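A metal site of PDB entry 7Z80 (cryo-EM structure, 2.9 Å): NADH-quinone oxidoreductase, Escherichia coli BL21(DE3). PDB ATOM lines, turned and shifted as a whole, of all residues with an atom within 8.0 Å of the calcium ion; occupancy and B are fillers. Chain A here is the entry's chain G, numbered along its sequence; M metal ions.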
ATOM      1  N   GLU A 615     -15.266 -27.260  34.641  1.00  0.00           N
ATOM      2  CA  GLU A 615     -16.100 -28.124  33.822  1.00  0.00           C
ATOM      3  C   GLU A 615     -17.417 -27.470  33.422  1.00  0.00           C
ATOM      4  O   GLU A 615     -18.310 -28.143  32.922  1.00  0.00           O
ATOM      5  CB  GLU A 615     -16.373 -29.438  34.552  1.00  0.00           C
ATOM      6  CG  GLU A 615     -15.132 -30.189  34.983  1.00  0.00           C
ATOM      7  CD  GLU A 615     -15.130 -30.543  36.450  1.00  0.00           C
ATOM      8  OE1 GLU A 615     -15.382 -29.647  37.284  1.00  0.00           O
ATOM      9  OE2 GLU A 615     -14.877 -31.715  36.777  1.00  0.00           O
ATOM     10  N   SER A 616     -17.555 -26.159  33.639  1.00  0.00           N
ATOM     11  CA  SER A 616     -18.791 -25.459  33.317  1.00  0.00           C
ATOM     12  C   SER A 616     -18.470 -24.104  32.693  1.00  0.00           C
ATOM     13  O   SER A 616     -17.409 -23.532  32.920  1.00  0.00           O
ATOM     14  CB  SER A 616     -19.665 -25.257  34.558  1.00  0.00           C
ATOM     15  OG  SER A 616     -19.414 -24.005  35.165  1.00  0.00           O
ATOM     16  N   ASP A 617     -19.411 -23.614  31.896  1.00  0.00           N
ATOM     17  CA  ASP A 617     -19.381 -22.267  31.359  1.00  0.00           C
ATOM     18  C   ASP A 617     -20.331 -21.384  32.165  1.00  0.00           C
ATOM     19  O   ASP A 617     -21.296 -21.875  32.764  1.00  0.00           O
ATOM     20  CB  ASP A 617     -19.795 -22.253  29.894  1.00  0.00           C
ATOM     21  CG  ASP A 617     -19.095 -23.318  29.088  1.00  0.00           C
ATOM     22  OD1 ASP A 617     -17.878 -23.182  28.852  1.00  0.00           O
ATOM     23  OD2 ASP A 617     -19.759 -24.303  28.697  1.00  0.00           O
ATOM     24  N   GLY A 618     -20.052 -20.097  32.194  1.00  0.00           N
ATOM     25  CA  GLY A 618     -20.930 -19.196  32.911  1.00  0.00           C
ATOM     26  C   GLY A 618     -20.392 -17.777  32.950  1.00  0.00           C
ATOM     27  O   GLY A 618     -19.392 -17.463  32.308  1.00  0.00           O
ATOM     28  N   PHE A 631     -15.123 -20.076  30.718  1.00  0.00           N
ATOM     29  CA  PHE A 631     -15.395 -21.132  29.755  1.00  0.00           C
ATOM     30  C   PHE A 631     -14.930 -22.480  30.311  1.00  0.00           C
ATOM     31  O   PHE A 631     -14.062 -22.554  31.182  1.00  0.00           O
ATOM     32  CB  PHE A 631     -14.677 -20.849  28.421  1.00  0.00           C
ATOM     33  CG  PHE A 631     -15.034 -19.522  27.801  1.00  0.00           C
ATOM     34  CD1 PHE A 631     -14.374 -18.362  28.167  1.00  0.00           C
ATOM     35  CD2 PHE A 631     -16.026 -19.439  26.842  1.00  0.00           C
ATOM     36  CE1 PHE A 631     -14.702 -17.151  27.598  1.00  0.00           C
ATOM     37  CE2 PHE A 631     -16.352 -18.232  26.264  1.00  0.00           C
ATOM     38  CZ  PHE A 631     -15.691 -17.086  26.647  1.00  0.00           C
ATOM     39  N   GLN A 632     -15.548 -23.543  29.796  1.00  0.00           N
ATOM     40  CA  GLN A 632     -15.212 -24.886  30.231  1.00  0.00           C
ATOM     41  C   GLN A 632     -13.828 -25.289  29.749  1.00  0.00           C
ATOM     42  O   GLN A 632     -13.427 -24.978  28.625  1.00  0.00           O
ATOM     43  CB  GLN A 632     -16.258 -25.878  29.708  1.00  0.00           C
ATOM     44  CG  GLN A 632     -16.058 -27.308  30.145  1.00  0.00           C
ATOM     45  CD  GLN A 632     -17.202 -28.208  29.717  1.00  0.00           C
ATOM     46  OE1 GLN A 632     -18.261 -27.734  29.316  1.00  0.00           O
ATOM     47  NE2 GLN A 632     -16.984 -29.515  29.792  1.00  0.00           N
ATOM     48  N   VAL A 633     -13.083 -25.967  30.616  1.00  0.00           N
ATOM     49  CA  VAL A 633     -11.725 -26.399  30.281  1.00  0.00           C
ATOM     50  C   VAL A 633     -11.725 -27.759  29.611  1.00  0.00           C
ATOM     51  O   VAL A 633     -11.040 -27.969  28.603  1.00  0.00           O
ATOM     52  CB  VAL A 633     -10.850 -26.400  31.554  1.00  0.00           C
ATOM     53  CG1 VAL A 633      -9.386 -26.544  31.188  1.00  0.00           C
ATOM     54  CG2 VAL A 633     -11.084 -25.143  32.352  1.00  0.00           C
ATOM     55  N   TYR A 634     -12.486 -28.706  30.149  1.00  0.00           N
ATOM     56  CA  TYR A 634     -12.469 -30.063  29.635  1.00  0.00           C
ATOM     57  C   TYR A 634     -13.828 -30.699  29.834  1.00  0.00           C
ATOM     58  O   TYR A 634     -14.629 -30.265  30.662  1.00  0.00           O
ATOM     59  CB  TYR A 634     -11.376 -30.914  30.300  1.00  0.00           C
ATOM     60  CG  TYR A 634     -11.564 -31.125  31.787  1.00  0.00           C
ATOM     61  CD1 TYR A 634     -11.227 -30.143  32.706  1.00  0.00           C
ATOM     62  CD2 TYR A 634     -12.074 -32.327  32.275  1.00  0.00           C
ATOM     63  CE1 TYR A 634     -11.397 -30.341  34.060  1.00  0.00           C
ATOM     64  CE2 TYR A 634     -12.244 -32.525  33.629  1.00  0.00           C
ATOM     65  CZ  TYR A 634     -11.904 -31.536  34.513  1.00  0.00           C
ATOM     66  OH  TYR A 634     -12.065 -31.732  35.868  1.00  0.00           O
ATOM     67  N   ASP A 635     -14.088 -31.744  29.046  1.00  0.00           N
ATOM     68  CA  ASP A 635     -15.278 -32.555  29.210  1.00  0.00           C
ATOM     69  C   ASP A 635     -15.006 -33.668  30.210  1.00  0.00           C
ATOM     70  O   ASP A 635     -14.099 -34.469  29.978  1.00  0.00           O
ATOM     71  CB  ASP A 635     -15.713 -33.137  27.871  1.00  0.00           C
ATOM     72  CG  ASP A 635     -17.096 -33.751  27.924  1.00  0.00           C
ATOM     73  OD1 ASP A 635     -18.048 -33.044  28.315  1.00  0.00           O
ATOM     74  OD2 ASP A 635     -17.233 -34.937  27.560  1.00  0.00           O
ATOM     75  N   PRO A 636     -15.740 -33.729  31.323  1.00  0.00           N
ATOM     76  CA  PRO A 636     -15.441 -34.771  32.324  1.00  0.00           C
ATOM     77  C   PRO A 636     -15.719 -36.181  31.849  1.00  0.00           C
ATOM     78  O   PRO A 636     -15.099 -37.127  32.362  1.00  0.00           O
ATOM     79  CB  PRO A 636     -16.364 -34.397  33.498  1.00  0.00           C
ATOM     80  CG  PRO A 636     -16.757 -32.973  33.249  1.00  0.00           C
ATOM     81  CD  PRO A 636     -16.788 -32.814  31.775  1.00  0.00           C
ATOM     82  N   LEU A 646     -22.915 -32.074  34.715  1.00  0.00           N
ATOM     83  CA  LEU A 646     -23.375 -31.055  33.794  1.00  0.00           C
ATOM     84  C   LEU A 646     -23.346 -29.688  34.469  1.00  0.00           C
ATOM     85  O   LEU A 646     -23.151 -29.572  35.678  1.00  0.00           O
ATOM     86  CB  LEU A 646     -24.796 -31.368  33.304  1.00  0.00           C
ATOM     87  CG  LEU A 646     -24.934 -32.659  32.486  1.00  0.00           C
ATOM     88  CD1 LEU A 646     -26.361 -33.163  32.530  1.00  0.00           C
ATOM     89  CD2 LEU A 646     -24.491 -32.420  31.049  1.00  0.00           C
ATOM     90  N   GLU A 647     -23.504 -28.657  33.647  1.00  0.00           N
ATOM     91  CA  GLU A 647     -23.613 -27.302  34.162  1.00  0.00           C
ATOM     92  C   GLU A 647     -24.860 -27.167  35.023  1.00  0.00           C
ATOM     93  O   GLU A 647     -25.894 -27.786  34.754  1.00  0.00           O
ATOM     94  CB  GLU A 647     -23.660 -26.307  33.008  1.00  0.00           C
ATOM     95  CG  GLU A 647     -22.339 -26.121  32.282  1.00  0.00           C
ATOM     96  CD  GLU A 647     -22.181 -27.043  31.085  1.00  0.00           C
ATOM     97  OE1 GLU A 647     -22.669 -28.195  31.141  1.00  0.00           O
ATOM     98  OE2 GLU A 647     -21.577 -26.615  30.085  1.00  0.00           O
ATOM     99  N   TRP A 649     -26.813 -24.542  35.520  1.00  0.00           N
ATOM    100  CA  TRP A 649     -27.900 -23.937  34.765  1.00  0.00           C
ATOM    101  C   TRP A 649     -28.516 -24.939  33.799  1.00  0.00           C
ATOM    102  O   TRP A 649     -29.734 -24.890  33.568  1.00  0.00           O
ATOM    103  CB  TRP A 649     -27.423 -22.694  34.023  1.00  0.00           C
ATOM    104  CG  TRP A 649     -26.168 -22.859  33.220  1.00  0.00           C
ATOM    105  CD1 TRP A 649     -24.892 -22.584  33.625  1.00  0.00           C
ATOM    106  CD2 TRP A 649     -26.070 -23.317  31.872  1.00  0.00           C
ATOM    107  NE1 TRP A 649     -24.008 -22.849  32.619  1.00  0.00           N
ATOM    108  CE2 TRP A 649     -24.695 -23.303  31.523  1.00  0.00           C
ATOM    109  CE3 TRP A 649     -26.990 -23.746  30.920  1.00  0.00           C
ATOM    110  CZ2 TRP A 649     -24.244 -23.695  30.277  1.00  0.00           C
ATOM    111  CZ3 TRP A 649     -26.538 -24.147  29.678  1.00  0.00           C
ATOM    112  CH2 TRP A 649     -25.173 -24.110  29.361  1.00  0.00           C
ATOM    113  N   ARG A 650     -27.721 -25.851  33.242  1.00  0.00           N
ATOM    114  CA  ARG A 650     -28.272 -26.901  32.398  1.00  0.00           C
ATOM    115  C   ARG A 650     -29.145 -27.858  33.210  1.00  0.00           C
ATOM    116  O   ARG A 650     -30.234 -28.243  32.761  1.00  0.00           O
ATOM    117  CB  ARG A 650     -27.148 -27.659  31.695  1.00  0.00           C
ATOM    118  CG  ARG A 650     -27.645 -28.623  30.644  1.00  0.00           C
ATOM    119  CD  ARG A 650     -26.500 -29.369  29.985  1.00  0.00           C
ATOM    120  NE  ARG A 650     -25.484 -28.462  29.468  1.00  0.00           N
ATOM    121  CZ  ARG A 650     -25.545 -27.854  28.285  1.00  0.00           C
ATOM    122  NH1 ARG A 650     -26.574 -28.032  27.473  1.00  0.00           N
ATOM    123  NH2 ARG A 650     -24.549 -27.052  27.914  1.00  0.00           N
ATOM    124  N   LEU A 669     -25.868 -22.314  26.172  1.00  0.00           N
ATOM    125  CA  LEU A 669     -25.467 -21.233  27.068  1.00  0.00           C
ATOM    126  C   LEU A 669     -26.050 -19.896  26.632  1.00  0.00           C
ATOM    127  O   LEU A 669     -26.488 -19.098  27.460  1.00  0.00           O
ATOM    128  CB  LEU A 669     -23.943 -21.156  27.146  1.00  0.00           C
ATOM    129  CG  LEU A 669     -23.372 -20.014  27.993  1.00  0.00           C
ATOM    130  CD1 LEU A 669     -23.695 -20.209  29.463  1.00  0.00           C
ATOM    131  CD2 LEU A 669     -21.867 -19.887  27.784  1.00  0.00           C
ATOM    132  N   ARG A 704      -8.495 -24.895  22.304  1.00  0.00           N
ATOM    133  CA  ARG A 704      -8.261 -25.009  23.733  1.00  0.00           C
ATOM    134  C   ARG A 704      -6.877 -25.541  24.058  1.00  0.00           C
ATOM    135  O   ARG A 704      -6.382 -25.308  25.172  1.00  0.00           O
ATOM    136  CB  ARG A 704      -9.319 -25.902  24.377  1.00  0.00           C
ATOM    137  CG  ARG A 704     -10.585 -25.191  24.790  1.00  0.00           C
ATOM    138  CD  ARG A 704     -11.445 -26.071  25.674  1.00  0.00           C
ATOM    139  NE  ARG A 704     -12.652 -25.383  26.143  1.00  0.00           N
ATOM    140  CZ  ARG A 704     -13.801 -25.360  25.488  1.00  0.00           C
ATOM    141  NH1 ARG A 704     -13.952 -25.994  24.336  1.00  0.00           N
ATOM    142  NH2 ARG A 704     -14.824 -24.691  25.997  1.00  0.00           N
ATOM    143  N   GLN A 728     -17.743 -32.079  21.710  1.00  0.00           N
ATOM    144  CA  GLN A 728     -18.218 -30.924  20.963  1.00  0.00           C
ATOM    145  C   GLN A 728     -18.686 -29.851  21.930  1.00  0.00           C
ATOM    146  O   GLN A 728     -19.463 -30.145  22.848  1.00  0.00           O
ATOM    147  CB  GLN A 728     -19.345 -31.309  20.010  1.00  0.00           C
ATOM    148  CG  GLN A 728     -18.950 -32.309  18.931  1.00  0.00           C
ATOM    149  CD  GLN A 728     -17.684 -31.923  18.204  1.00  0.00           C
ATOM    150  OE1 GLN A 728     -17.668 -30.961  17.439  1.00  0.00           O
ATOM    151  NE2 GLN A 728     -16.618 -32.679  18.430  1.00  0.00           N
ATOM    152  N   ASP A 729     -18.223 -28.632  21.733  1.00  0.00           N
ATOM    153  CA  ASP A 729     -18.613 -27.492  22.571  1.00  0.00           C
ATOM    154  C   ASP A 729     -19.697 -26.727  21.831  1.00  0.00           C
ATOM    155  O   ASP A 729     -19.413 -25.915  20.948  1.00  0.00           O
ATOM    156  CB  ASP A 729     -17.407 -26.602  22.875  1.00  0.00           C
ATOM    157  CG  ASP A 729     -17.643 -25.702  24.074  1.00  0.00           C
ATOM    158  OD1 ASP A 729     -18.671 -25.878  24.766  1.00  0.00           O
ATOM    159  OD2 ASP A 729     -16.799 -24.818  24.315  1.00  0.00           O
ATOM    160  N   ILE A 730     -20.956 -26.991  22.195  1.00  0.00           N
ATOM    161  CA  ILE A 730     -22.064 -26.233  21.628  1.00  0.00           C
ATOM    162  C   ILE A 730     -22.321 -24.941  22.385  1.00  0.00           C
ATOM    163  O   ILE A 730     -23.070 -24.082  21.897  1.00  0.00           O
ATOM    164  CB  ILE A 730     -23.351 -27.086  21.599  1.00  0.00           C
ATOM    165  CG1 ILE A 730     -23.819 -27.389  23.022  1.00  0.00           C
ATOM    166  CG2 ILE A 730     -23.124 -28.368  20.821  1.00  0.00           C
ATOM    167  CD1 ILE A 730     -25.235 -27.875  23.105  1.00  0.00           C
ATOM    168  N   ASP A 731     -21.719 -24.765  23.558  1.00  0.00           N
ATOM    169  CA  ASP A 731     -21.990 -23.598  24.392  1.00  0.00           C
ATOM    170  C   ASP A 731     -21.171 -22.392  23.977  1.00  0.00           C
ATOM    171  O   ASP A 731     -21.706 -21.274  23.889  1.00  0.00           O
ATOM    172  CB  ASP A 731     -21.723 -23.931  25.859  1.00  0.00           C
ATOM    173  CG  ASP A 731     -22.701 -24.938  26.412  1.00  0.00           C
ATOM    174  OD1 ASP A 731     -23.871 -24.930  25.989  1.00  0.00           O
ATOM    175  OD2 ASP A 731     -22.298 -25.750  27.272  1.00  0.00           O
ATOM    176  N   THR A 732     -19.882 -22.570  23.725  1.00  0.00           N
ATOM    177  CA  THR A 732     -18.970 -21.469  23.471  1.00  0.00           C
ATOM    178  C   THR A 732     -18.401 -21.574  22.054  1.00  0.00           C
ATOM    179  O   THR A 732     -18.728 -22.470  21.280  1.00  0.00           O
ATOM    180  CB  THR A 732     -17.822 -21.450  24.482  1.00  0.00           C
ATOM    181  OG1 THR A 732     -16.711 -22.185  23.965  1.00  0.00           O
ATOM    182  CG2 THR A 732     -18.257 -22.066  25.804  1.00  0.00           C
ATOM    183  N   PHE A 736     -12.744 -28.370  21.886  1.00  0.00           N
ATOM    184  CA  PHE A 736     -11.908 -29.239  22.706  1.00  0.00           C
ATOM    185  C   PHE A 736     -10.856 -29.955  21.870  1.00  0.00           C
ATOM    186  O   PHE A 736     -10.748 -31.185  21.933  1.00  0.00           O
ATOM    187  CB  PHE A 736     -12.763 -30.276  23.454  1.00  0.00           C
ATOM    188  CG  PHE A 736     -13.701 -29.678  24.461  1.00  0.00           C
ATOM    189  CD1 PHE A 736     -13.232 -29.275  25.701  1.00  0.00           C
ATOM    190  CD2 PHE A 736     -15.046 -29.530  24.173  1.00  0.00           C
ATOM    191  CE1 PHE A 736     -14.095 -28.729  26.636  1.00  0.00           C
ATOM    192  CE2 PHE A 736     -15.915 -28.999  25.101  1.00  0.00           C
ATOM    193  CZ  PHE A 736     -15.436 -28.588  26.329  1.00  0.00           C
HETATM  194 CA    CA M   1     -20.182 -26.833  28.018  1.00  0.00          CA
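The calcium ion is bound by the side-chain amide oxygen (OE1) of Gln 632 (2.5 Å).
The calcium ion is bound by OD2 of Asp 731.
The calcium ion is bound by the side-chain carboxylate (OE2) of Glu 647, 2.5 Å away.
The calcium ion is bound by the side-chain carboxylate (OD2) of Asp 617 (2.7 Å).
OD1 of Asp 729 touches the calcium ion, at 3.7 Å.
Five residues have an atom within 4 Å of the calcium ion: Asp 617, Gln 632, Glu 647, Asp 729 and Asp 731.
The backbone carbonyl oxygen (O) of Asp 617 is in hydrogen-bond range of the indole nitrogen (NE1) of Trp 649 (2.9 Å).
The side-chain carboxylate (OE1) of Glu 647 is in salt-bridge range of the guanidinium group (NE) of Arg 650.
The side-chain carboxylate (OD2) of Asp 729 lies within salt-bridge range of the guanidinium group (NH2) of Arg 704, 2.6 Å away.
The side-chain carboxylate of Asp 729 is in hydrogen-bond range of the side-chain hydroxyl of Thr 732, at 2.7 Å.
The side-chain carboxylate (OD1) of Asp 731 is in hydrogen-bond range of the backbone NH (N) of Leu 669 (3.3 Å).
The side-chain carboxylate of Asp 729 sits close to the backbone NH of Asp 731 (3.5 Å).
The side-chain amide nitrogen (NE2) of Gln 632 lies within hydrogen-bond range of the backbone carbonyl oxygen (O) of Tyr 634 (2.6 Å).
NH2 of Arg 650 is in salt-bridge range of OD1 of Asp 731, at 2.9 Å.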
